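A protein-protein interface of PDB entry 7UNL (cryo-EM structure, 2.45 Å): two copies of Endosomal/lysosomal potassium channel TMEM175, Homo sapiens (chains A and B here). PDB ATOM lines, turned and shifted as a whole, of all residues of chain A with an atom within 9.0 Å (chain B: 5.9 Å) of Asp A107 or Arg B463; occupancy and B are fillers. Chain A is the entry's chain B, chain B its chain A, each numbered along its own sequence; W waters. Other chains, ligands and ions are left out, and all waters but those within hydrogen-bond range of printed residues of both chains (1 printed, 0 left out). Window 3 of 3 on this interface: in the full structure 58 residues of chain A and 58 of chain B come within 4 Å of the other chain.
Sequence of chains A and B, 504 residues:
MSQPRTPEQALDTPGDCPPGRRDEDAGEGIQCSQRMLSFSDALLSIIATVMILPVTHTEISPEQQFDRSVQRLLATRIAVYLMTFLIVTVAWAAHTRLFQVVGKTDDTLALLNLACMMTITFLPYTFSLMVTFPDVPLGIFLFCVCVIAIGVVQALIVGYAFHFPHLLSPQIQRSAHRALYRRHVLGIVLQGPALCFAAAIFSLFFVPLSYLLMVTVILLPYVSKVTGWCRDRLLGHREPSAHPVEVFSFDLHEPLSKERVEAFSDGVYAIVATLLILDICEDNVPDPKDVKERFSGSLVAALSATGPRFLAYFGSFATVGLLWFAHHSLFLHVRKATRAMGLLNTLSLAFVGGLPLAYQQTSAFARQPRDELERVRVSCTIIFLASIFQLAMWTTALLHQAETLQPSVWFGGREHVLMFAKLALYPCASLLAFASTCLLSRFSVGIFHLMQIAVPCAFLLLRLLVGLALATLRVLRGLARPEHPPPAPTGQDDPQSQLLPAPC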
ATOM      1  N   ILE A  30       0.936 -34.609  24.813  1.00  0.00           N
ATOM      2  CA  ILE A  30       2.233 -35.018  24.289  1.00  0.00           C
ATOM      3  C   ILE A  30       2.042 -36.163  23.302  1.00  0.00           C
ATOM      4  O   ILE A  30       1.193 -37.029  23.501  1.00  0.00           O
ATOM      5  CB  ILE A  30       3.192 -35.406  25.422  1.00  0.00           C
ATOM      6  CG1 ILE A  30       2.597 -36.527  26.277  1.00  0.00           C
ATOM      7  CG2 ILE A  30       3.506 -34.188  26.273  1.00  0.00           C
ATOM      8  CD1 ILE A  30       3.220 -37.877  26.018  1.00  0.00           C
ATOM      9  N   GLN A  31       2.846 -36.161  22.240  1.00  0.00           N
ATOM     10  CA  GLN A  31       2.582 -36.999  21.081  1.00  0.00           C
ATOM     11  C   GLN A  31       3.880 -37.614  20.577  1.00  0.00           C
ATOM     12  O   GLN A  31       4.971 -37.091  20.824  1.00  0.00           O
ATOM     13  CB  GLN A  31       1.934 -36.197  19.942  1.00  0.00           C
ATOM     14  CG  GLN A  31       0.904 -35.152  20.373  1.00  0.00           C
ATOM     15  CD  GLN A  31       0.812 -33.988  19.405  1.00  0.00           C
ATOM     16  OE1 GLN A  31       1.596 -33.884  18.461  1.00  0.00           O
ATOM     17  NE2 GLN A  31      -0.149 -33.103  19.636  1.00  0.00           N
ATOM     18  N   MET A  36       5.318 -36.151  12.220  1.00  0.00           N
ATOM     19  CA  MET A  36       5.789 -34.790  12.002  1.00  0.00           C
ATOM     20  C   MET A  36       7.163 -34.787  11.343  1.00  0.00           C
ATOM     21  O   MET A  36       7.419 -34.000  10.423  1.00  0.00           O
ATOM     22  CB  MET A  36       5.817 -34.040  13.333  1.00  0.00           C
ATOM     23  CG  MET A  36       6.207 -32.578  13.223  1.00  0.00           C
ATOM     24  SD  MET A  36       6.482 -31.797  14.824  1.00  0.00           S
ATOM     25  CE  MET A  36       8.026 -32.549  15.319  1.00  0.00           C
ATOM     26  N   LYS A 104       9.687 -36.420  22.106  1.00  0.00           N
ATOM     27  CA  LYS A 104       8.246 -36.320  21.949  1.00  0.00           C
ATOM     28  C   LYS A 104       7.856 -34.880  21.643  1.00  0.00           C
ATOM     29  O   LYS A 104       8.484 -33.938  22.134  1.00  0.00           O
ATOM     30  CB  LYS A 104       7.529 -36.807  23.209  1.00  0.00           C
ATOM     31  CG  LYS A 104       7.314 -38.315  23.243  1.00  0.00           C
ATOM     32  CD  LYS A 104       6.114 -38.715  24.091  1.00  0.00           C
ATOM     33  CE  LYS A 104       6.534 -39.197  25.470  1.00  0.00           C
ATOM     34  NZ  LYS A 104       6.962 -38.075  26.347  1.00  0.00           N
ATOM     35  N   THR A 105       6.824 -34.719  20.823  1.00  0.00           N
ATOM     36  CA  THR A 105       6.367 -33.415  20.367  1.00  0.00           C
ATOM     37  C   THR A 105       5.006 -33.079  20.963  1.00  0.00           C
ATOM     38  O   THR A 105       4.324 -33.921  21.551  1.00  0.00           O
ATOM     39  CB  THR A 105       6.295 -33.368  18.834  1.00  0.00           C
ATOM     40  OG1 THR A 105       5.858 -32.072  18.412  1.00  0.00           O
ATOM     41  CG2 THR A 105       5.337 -34.425  18.295  1.00  0.00           C
ATOM     42  N   ASP A 106       4.625 -31.817  20.804  1.00  0.00           N
ATOM     43  CA  ASP A 106       3.314 -31.336  21.219  1.00  0.00           C
ATOM     44  C   ASP A 106       2.826 -30.352  20.158  1.00  0.00           C
ATOM     45  O   ASP A 106       3.451 -30.160  19.107  1.00  0.00           O
ATOM     46  CB  ASP A 106       3.387 -30.729  22.627  1.00  0.00           C
ATOM     47  CG  ASP A 106       4.070 -29.379  22.650  1.00  0.00           C
ATOM     48  OD1 ASP A 106       5.312 -29.336  22.521  1.00  0.00           O
ATOM     49  OD2 ASP A 106       3.367 -28.358  22.799  1.00  0.00           O
ATOM     50  N   ASP A 107       1.686 -29.713  20.422  1.00  0.00           N
ATOM     51  CA  ASP A 107       1.096 -28.801  19.446  1.00  0.00           C
ATOM     52  C   ASP A 107       2.017 -27.619  19.166  1.00  0.00           C
ATOM     53  O   ASP A 107       2.261 -27.261  18.004  1.00  0.00           O
ATOM     54  CB  ASP A 107      -0.260 -28.314  19.957  1.00  0.00           C
ATOM     55  CG  ASP A 107      -1.367 -29.325  19.734  1.00  0.00           C
ATOM     56  OD1 ASP A 107      -1.151 -30.296  18.981  1.00  0.00           O
ATOM     57  OD2 ASP A 107      -2.456 -29.147  20.318  1.00  0.00           O
ATOM     58  N   THR A 108       2.543 -27.002  20.227  1.00  0.00           N
ATOM     59  CA  THR A 108       3.410 -25.844  20.058  1.00  0.00           C
ATOM     60  C   THR A 108       4.642 -26.201  19.239  1.00  0.00           C
ATOM     61  O   THR A 108       5.054 -25.438  18.358  1.00  0.00           O
ATOM     62  CB  THR A 108       3.818 -25.296  21.424  1.00  0.00           C
ATOM     63  OG1 THR A 108       2.688 -25.314  22.305  1.00  0.00           O
ATOM     64  CG2 THR A 108       4.336 -23.876  21.302  1.00  0.00           C
ATOM     65  N   LEU A 109       5.241 -27.360  19.514  1.00  0.00           N
ATOM     66  CA  LEU A 109       6.426 -27.765  18.773  1.00  0.00           C
ATOM     67  C   LEU A 109       6.103 -28.066  17.317  1.00  0.00           C
ATOM     68  O   LEU A 109       6.921 -27.785  16.438  1.00  0.00           O
ATOM     69  CB  LEU A 109       7.073 -28.975  19.441  1.00  0.00           C
ATOM     70  CG  LEU A 109       7.878 -28.651  20.698  1.00  0.00           C
ATOM     71  CD1 LEU A 109       8.363 -29.922  21.364  1.00  0.00           C
ATOM     72  CD2 LEU A 109       9.044 -27.742  20.368  1.00  0.00           C
ATOM     73  N   ALA A 110       4.928 -28.629  17.037  1.00  0.00           N
ATOM     74  CA  ALA A 110       4.535 -28.845  15.649  1.00  0.00           C
ATOM     75  C   ALA A 110       4.389 -27.524  14.902  1.00  0.00           C
ATOM     76  O   ALA A 110       4.861 -27.388  13.766  1.00  0.00           O
ATOM     77  CB  ALA A 110       3.236 -29.643  15.596  1.00  0.00           C
ATOM     78  N   LEU A 111       3.744 -26.536  15.523  1.00  0.00           N
ATOM     79  CA  LEU A 111       3.609 -25.233  14.880  1.00  0.00           C
ATOM     80  C   LEU A 111       4.973 -24.579  14.671  1.00  0.00           C
ATOM     81  O   LEU A 111       5.245 -23.990  13.615  1.00  0.00           O
ATOM     82  CB  LEU A 111       2.695 -24.341  15.719  1.00  0.00           C
ATOM     83  CG  LEU A 111       1.269 -24.876  15.881  1.00  0.00           C
ATOM     84  CD1 LEU A 111       0.452 -23.998  16.808  1.00  0.00           C
ATOM     85  CD2 LEU A 111       0.590 -25.007  14.536  1.00  0.00           C
ATOM     86  N   LEU A 112       5.849 -24.678  15.671  1.00  0.00           N
ATOM     87  CA  LEU A 112       7.188 -24.116  15.547  1.00  0.00           C
ATOM     88  C   LEU A 112       7.979 -24.809  14.444  1.00  0.00           C
ATOM     89  O   LEU A 112       8.743 -24.167  13.716  1.00  0.00           O
ATOM     90  CB  LEU A 112       7.911 -24.223  16.887  1.00  0.00           C
ATOM     91  CG  LEU A 112       7.613 -23.093  17.875  1.00  0.00           C
ATOM     92  CD1 LEU A 112       8.184 -23.415  19.246  1.00  0.00           C
ATOM     93  CD2 LEU A 112       8.147 -21.767  17.362  1.00  0.00           C
ATOM     94  N   ASN A 113       7.814 -26.126  14.310  1.00  0.00           N
ATOM     95  CA  ASN A 113       8.477 -26.854  13.236  1.00  0.00           C
ATOM     96  C   ASN A 113       7.944 -26.426  11.876  1.00  0.00           C
ATOM     97  O   ASN A 113       8.697 -26.362  10.900  1.00  0.00           O
ATOM     98  CB  ASN A 113       8.298 -28.358  13.439  1.00  0.00           C
ATOM     99  CG  ASN A 113       8.965 -29.173  12.354  1.00  0.00           C
ATOM    100  OD1 ASN A 113      10.183 -29.133  12.194  1.00  0.00           O
ATOM    101  ND2 ASN A 113       8.169 -29.913  11.597  1.00  0.00           N
ATOM    102  N   LEU A 114       6.643 -26.146  11.787  1.00  0.00           N
ATOM    103  CA  LEU A 114       6.103 -25.590  10.549  1.00  0.00           C
ATOM    104  C   LEU A 114       6.759 -24.255  10.222  1.00  0.00           C
ATOM    105  O   LEU A 114       7.108 -23.988   9.064  1.00  0.00           O
ATOM    106  CB  LEU A 114       4.590 -25.422  10.659  1.00  0.00           C
ATOM    107  CG  LEU A 114       3.755 -26.693  10.509  1.00  0.00           C
ATOM    108  CD1 LEU A 114       2.335 -26.439  10.974  1.00  0.00           C
ATOM    109  CD2 LEU A 114       3.775 -27.181   9.069  1.00  0.00           C
ATOM    110  N   TYR A 160      11.756 -24.165  24.428  1.00  0.00           N
ATOM    111  CA  TYR A 160      10.451 -24.687  24.814  1.00  0.00           C
ATOM    112  C   TYR A 160      10.565 -26.115  25.328  1.00  0.00           C
ATOM    113  O   TYR A 160       9.958 -26.464  26.347  1.00  0.00           O
ATOM    114  CB  TYR A 160       9.490 -24.631  23.627  1.00  0.00           C
ATOM    115  CG  TYR A 160       8.095 -25.116  23.945  1.00  0.00           C
ATOM    116  CD1 TYR A 160       7.125 -24.239  24.401  1.00  0.00           C
ATOM    117  CD2 TYR A 160       7.754 -26.453  23.805  1.00  0.00           C
ATOM    118  CE1 TYR A 160       5.850 -24.674  24.691  1.00  0.00           C
ATOM    119  CE2 TYR A 160       6.484 -26.899  24.101  1.00  0.00           C
ATOM    120  CZ  TYR A 160       5.536 -26.006  24.545  1.00  0.00           C
ATOM    121  OH  TYR A 160       4.266 -26.445  24.839  1.00  0.00           O
ATOM    122  N   LEU A 167       9.302 -33.422  27.348  1.00  0.00           N
ATOM    123  CA  LEU A 167       9.404 -33.507  25.898  1.00  0.00           C
ATOM    124  C   LEU A 167      10.805 -33.869  25.424  1.00  0.00           C
ATOM    125  O   LEU A 167      10.999 -34.081  24.223  1.00  0.00           O
ATOM    126  CB  LEU A 167       8.985 -32.180  25.261  1.00  0.00           C
ATOM    127  CG  LEU A 167       7.498 -31.840  25.330  1.00  0.00           C
ATOM    128  CD1 LEU A 167       7.290 -30.362  25.068  1.00  0.00           C
ATOM    129  CD2 LEU A 167       6.706 -32.677  24.344  1.00  0.00           C
ATOM    130  N   PHE B 325      -1.838 -29.842  10.212  1.00  0.00           N
ATOM    131  CA  PHE B 325      -1.779 -29.922  11.665  1.00  0.00           C
ATOM    132  C   PHE B 325      -3.059 -30.526  12.231  1.00  0.00           C
ATOM    133  O   PHE B 325      -3.012 -31.398  13.107  1.00  0.00           O
ATOM    134  CB  PHE B 325      -1.521 -28.522  12.228  1.00  0.00           C
ATOM    135  CG  PHE B 325      -1.653 -28.419  13.718  1.00  0.00           C
ATOM    136  CD1 PHE B 325      -0.618 -28.814  14.545  1.00  0.00           C
ATOM    137  CD2 PHE B 325      -2.799 -27.897  14.293  1.00  0.00           C
ATOM    138  CE1 PHE B 325      -0.730 -28.709  15.914  1.00  0.00           C
ATOM    139  CE2 PHE B 325      -2.913 -27.790  15.663  1.00  0.00           C
ATOM    140  CZ  PHE B 325      -1.879 -28.197  16.472  1.00  0.00           C
ATOM    141  N   SER B 329      -3.311 -34.123  14.113  1.00  0.00           N
ATOM    142  CA  SER B 329      -3.914 -34.265  15.432  1.00  0.00           C
ATOM    143  C   SER B 329      -5.032 -35.300  15.415  1.00  0.00           C
ATOM    144  O   SER B 329      -5.156 -36.101  16.349  1.00  0.00           O
ATOM    145  CB  SER B 329      -4.438 -32.914  15.915  1.00  0.00           C
ATOM    146  OG  SER B 329      -3.442 -31.914  15.820  1.00  0.00           O
ATOM    147  N   GLU B 415      -9.949 -34.953  25.482  1.00  0.00           N
ATOM    148  CA  GLU B 415      -9.552 -34.256  24.265  1.00  0.00           C
ATOM    149  C   GLU B 415     -10.674 -34.164  23.237  1.00  0.00           C
ATOM    150  O   GLU B 415     -10.427 -33.744  22.103  1.00  0.00           O
ATOM    151  CB  GLU B 415      -8.336 -34.951  23.648  1.00  0.00           C
ATOM    152  CG  GLU B 415      -7.009 -34.543  24.262  1.00  0.00           C
ATOM    153  CD  GLU B 415      -6.050 -33.953  23.247  1.00  0.00           C
ATOM    154  OE1 GLU B 415      -6.490 -33.131  22.415  1.00  0.00           O
ATOM    155  OE2 GLU B 415      -4.853 -34.311  23.279  1.00  0.00           O
ATOM    156  N   LEU B 418     -11.474 -30.321  22.525  1.00  0.00           N
ATOM    157  CA  LEU B 418     -10.340 -29.691  21.858  1.00  0.00           C
ATOM    158  C   LEU B 418     -10.205 -30.183  20.424  1.00  0.00           C
ATOM    159  O   LEU B 418      -9.926 -29.395  19.514  1.00  0.00           O
ATOM    160  CB  LEU B 418      -9.054 -29.953  22.642  1.00  0.00           C
ATOM    161  CG  LEU B 418      -7.825 -29.195  22.136  1.00  0.00           C
ATOM    162  CD1 LEU B 418      -7.953 -27.706  22.419  1.00  0.00           C
ATOM    163  CD2 LEU B 418      -6.568 -29.747  22.758  1.00  0.00           C
ATOM    164  N   LYS B 422     -10.474 -27.918  17.099  1.00  0.00           N
ATOM    165  CA  LYS B 422      -9.382 -27.902  16.134  1.00  0.00           C
ATOM    166  C   LYS B 422      -9.884 -28.197  14.729  1.00  0.00           C
ATOM    167  O   LYS B 422      -9.448 -27.562  13.761  1.00  0.00           O
ATOM    168  CB  LYS B 422      -8.319 -28.917  16.549  1.00  0.00           C
ATOM    169  CG  LYS B 422      -6.940 -28.669  15.973  1.00  0.00           C
ATOM    170  CD  LYS B 422      -5.928 -29.627  16.569  1.00  0.00           C
ATOM    171  CE  LYS B 422      -5.513 -29.194  17.962  1.00  0.00           C
ATOM    172  NZ  LYS B 422      -4.723 -30.230  18.670  1.00  0.00           N
ATOM    173  N   ALA B 458      -5.239 -18.576  16.810  1.00  0.00           N
ATOM    174  CA  ALA B 458      -6.200 -19.411  17.524  1.00  0.00           C
ATOM    175  C   ALA B 458      -5.681 -20.834  17.681  1.00  0.00           C
ATOM    176  O   ALA B 458      -5.819 -21.437  18.752  1.00  0.00           O
ATOM    177  CB  ALA B 458      -7.541 -19.405  16.794  1.00  0.00           C
ATOM    178  N   PHE B 459      -5.085 -21.392  16.624  1.00  0.00           N
ATOM    179  CA  PHE B 459      -4.449 -22.698  16.755  1.00  0.00           C
ATOM    180  C   PHE B 459      -3.356 -22.671  17.812  1.00  0.00           C
ATOM    181  O   PHE B 459      -3.186 -23.640  18.559  1.00  0.00           O
ATOM    182  CB  PHE B 459      -3.865 -23.143  15.415  1.00  0.00           C
ATOM    183  CG  PHE B 459      -4.856 -23.803  14.507  1.00  0.00           C
ATOM    184  CD1 PHE B 459      -5.364 -25.053  14.808  1.00  0.00           C
ATOM    185  CD2 PHE B 459      -5.272 -23.179  13.345  1.00  0.00           C
ATOM    186  CE1 PHE B 459      -6.270 -25.664  13.971  1.00  0.00           C
ATOM    187  CE2 PHE B 459      -6.179 -23.786  12.507  1.00  0.00           C
ATOM    188  CZ  PHE B 459      -6.679 -25.030  12.820  1.00  0.00           C
ATOM    189  N   LEU B 460      -2.605 -21.571  17.885  1.00  0.00           N
ATOM    190  CA  LEU B 460      -1.537 -21.458  18.871  1.00  0.00           C
ATOM    191  C   LEU B 460      -2.085 -21.451  20.294  1.00  0.00           C
ATOM    192  O   LEU B 460      -1.507 -22.076  21.189  1.00  0.00           O
ATOM    193  CB  LEU B 460      -0.725 -20.194  18.597  1.00  0.00           C
ATOM    194  CG  LEU B 460       0.445 -19.867  19.525  1.00  0.00           C
ATOM    195  CD1 LEU B 460       1.367 -21.061  19.692  1.00  0.00           C
ATOM    196  CD2 LEU B 460       1.207 -18.672  18.980  1.00  0.00           C
ATOM    197  N   LEU B 461      -3.196 -20.748  20.525  1.00  0.00           N
ATOM    198  CA  LEU B 461      -3.784 -20.604  21.853  1.00  0.00           C
ATOM    199  C   LEU B 461      -5.098 -21.366  21.982  1.00  0.00           C
ATOM    200  O   LEU B 461      -5.977 -20.972  22.751  1.00  0.00           O
ATOM    201  CB  LEU B 461      -4.012 -19.129  22.178  1.00  0.00           C
ATOM    202  CG  LEU B 461      -2.896 -18.138  21.851  1.00  0.00           C
ATOM    203  CD1 LEU B 461      -3.455 -16.729  21.834  1.00  0.00           C
ATOM    204  CD2 LEU B 461      -1.757 -18.251  22.847  1.00  0.00           C
ATOM    205  N   LEU B 462      -5.249 -22.461  21.236  1.00  0.00           N
ATOM    206  CA  LEU B 462      -6.528 -23.160  21.203  1.00  0.00           C
ATOM    207  C   LEU B 462      -6.895 -23.729  22.568  1.00  0.00           C
ATOM    208  O   LEU B 462      -8.059 -23.669  22.976  1.00  0.00           O
ATOM    209  CB  LEU B 462      -6.486 -24.272  20.159  1.00  0.00           C
ATOM    210  CG  LEU B 462      -7.841 -24.867  19.780  1.00  0.00           C
ATOM    211  CD1 LEU B 462      -8.674 -23.868  18.999  1.00  0.00           C
ATOM    212  CD2 LEU B 462      -7.647 -26.138  18.984  1.00  0.00           C
ATOM    213  N   ARG B 463      -5.924 -24.302  23.280  1.00  0.00           N
ATOM    214  CA  ARG B 463      -6.226 -24.943  24.556  1.00  0.00           C
ATOM    215  C   ARG B 463      -6.749 -23.931  25.571  1.00  0.00           C
ATOM    216  O   ARG B 463      -7.757 -24.174  26.249  1.00  0.00           O
ATOM    217  CB  ARG B 463      -4.979 -25.649  25.089  1.00  0.00           C
ATOM    218  CG  ARG B 463      -5.238 -27.026  25.677  1.00  0.00           C
ATOM    219  CD  ARG B 463      -3.957 -27.842  25.769  1.00  0.00           C
ATOM    220  NE  ARG B 463      -3.560 -28.389  24.475  1.00  0.00           N
ATOM    221  CZ  ARG B 463      -3.683 -29.661  24.115  1.00  0.00           C
ATOM    222  NH1 ARG B 463      -4.190 -30.571  24.931  1.00  0.00           N
ATOM    223  NH2 ARG B 463      -3.291 -30.029  22.898  1.00  0.00           N
ATOM    224  N   LEU B 464      -6.072 -22.787  25.692  1.00  0.00           N
ATOM    225  CA  LEU B 464      -6.508 -21.769  26.641  1.00  0.00           C
ATOM    226  C   LEU B 464      -7.881 -21.222  26.270  1.00  0.00           C
ATOM    227  O   LEU B 464      -8.725 -21.000  27.144  1.00  0.00           O
ATOM    228  CB  LEU B 464      -5.484 -20.637  26.706  1.00  0.00           C
ATOM    229  CG  LEU B 464      -4.069 -21.036  27.126  1.00  0.00           C
ATOM    230  CD1 LEU B 464      -3.143 -19.837  27.043  1.00  0.00           C
ATOM    231  CD2 LEU B 464      -4.061 -21.626  28.529  1.00  0.00           C
ATOM    232  N   LEU B 465      -8.117 -20.988  24.978  1.00  0.00           N
ATOM    233  CA  LEU B 465      -9.418 -20.494  24.542  1.00  0.00           C
ATOM    234  C   LEU B 465     -10.520 -21.502  24.844  1.00  0.00           C
ATOM    235  O   LEU B 465     -11.617 -21.127  25.278  1.00  0.00           O
ATOM    236  CB  LEU B 465      -9.377 -20.171  23.048  1.00  0.00           C
ATOM    237  CG  LEU B 465      -8.500 -18.980  22.658  1.00  0.00           C
ATOM    238  CD1 LEU B 465      -8.029 -19.087  21.212  1.00  0.00           C
ATOM    239  CD2 LEU B 465      -9.250 -17.680  22.879  1.00  0.00           C
ATOM    240  N   VAL B 466     -10.249 -22.788  24.617  1.00  0.00           N
ATOM    241  CA  VAL B 466     -11.236 -23.825  24.905  1.00  0.00           C
ATOM    242  C   VAL B 466     -11.544 -23.857  26.395  1.00  0.00           C
ATOM    243  O   VAL B 466     -12.708 -23.946  26.807  1.00  0.00           O
ATOM    244  CB  VAL B 466     -10.738 -25.191  24.400  1.00  0.00           C
ATOM    245  CG1 VAL B 466     -11.366 -26.327  25.191  1.00  0.00           C
ATOM    246  CG2 VAL B 466     -11.032 -25.346  22.922  1.00  0.00           C
ATOM    247  N   GLY B 467     -10.503 -23.797  27.227  1.00  0.00           N
ATOM    248  CA  GLY B 467     -10.728 -23.773  28.664  1.00  0.00           C
ATOM    249  C   GLY B 467     -11.532 -22.563  29.101  1.00  0.00           C
ATOM    250  O   GLY B 467     -12.435 -22.670  29.936  1.00  0.00           O
ATOM    251  N   LEU B 468     -11.215 -21.395  28.539  1.00  0.00           N
ATOM    252  CA  LEU B 468     -11.943 -20.179  28.879  1.00  0.00           C
ATOM    253  C   LEU B 468     -13.411 -20.299  28.500  1.00  0.00           C
ATOM    254  O   LEU B 468     -14.298 -19.941  29.283  1.00  0.00           O
ATOM    255  CB  LEU B 468     -11.300 -18.981  28.180  1.00  0.00           C
ATOM    256  CG  LEU B 468     -11.944 -17.610  28.404  1.00  0.00           C
ATOM    257  CD1 LEU B 468     -10.877 -16.528  28.408  1.00  0.00           C
ATOM    258  CD2 LEU B 468     -12.997 -17.310  27.344  1.00  0.00           C
HETATM  259  O   HOH W   1      -0.917 -31.851  15.903  1.00  0.00           O
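The side-chain amino group (NZ) of Lys B422 lies within salt-bridge range of the side-chain carboxylate (OD2) of Asp A107, 3.0 Å away. The guanidinium group (NH2) of Arg B463 lies within salt-bridge range of the side-chain carboxylate (OD2) of Asp A107, at 2.9 Å.
Of the printed residues of chain B, Leu A111 touches Phe B325 (3.99 Å) and Leu B460 (3.8 Å). Of the printed residues of chain A, Lys B422 touches Asp A107. Gln A31 touches none of the printed residues of chain B. Met A36 touches none of the printed residues of chain B. The nearest residue of chain B that does not touch Asp A107 is Ser B329 (4.2 Å). The nearest residue of chain A that does not touch Arg B463 is Gln A31 (5.5 Å).
No position is printed for both chains. Of the 5 pairs that touch across the chains among the printed residues, none has its exchanged pair printed and touching as well.
Among the printed residues, pairs that only touch across the chains: Asp A107 with Phe B325 (3.4 Å), Leu A111 with Leu B460 (3.8 Å) and Leu A111 with Phe B325 (3.99 Å).
Water W1 bridges the side-chain hydroxyl (OG) of Ser B329 and the side-chain carboxylate (OD1) of Asp A107.
Hydrophobic or aromatic side chains of chain B within 4 Å of the printed part of chain A: Phe B325. Hydrophobic or aromatic side chains of chain A within 4 Å of the printed part of chain B: Leu A111. Among the printed residues, 5 pairs touch across the chains.
O of Phe B325 is in hydrogen-bond range of OG of Ser B329 (2.8 Å). NE2 of Gln A31 lies within hydrogen-bond range of OD1 of Asp A107 (3.1 Å).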
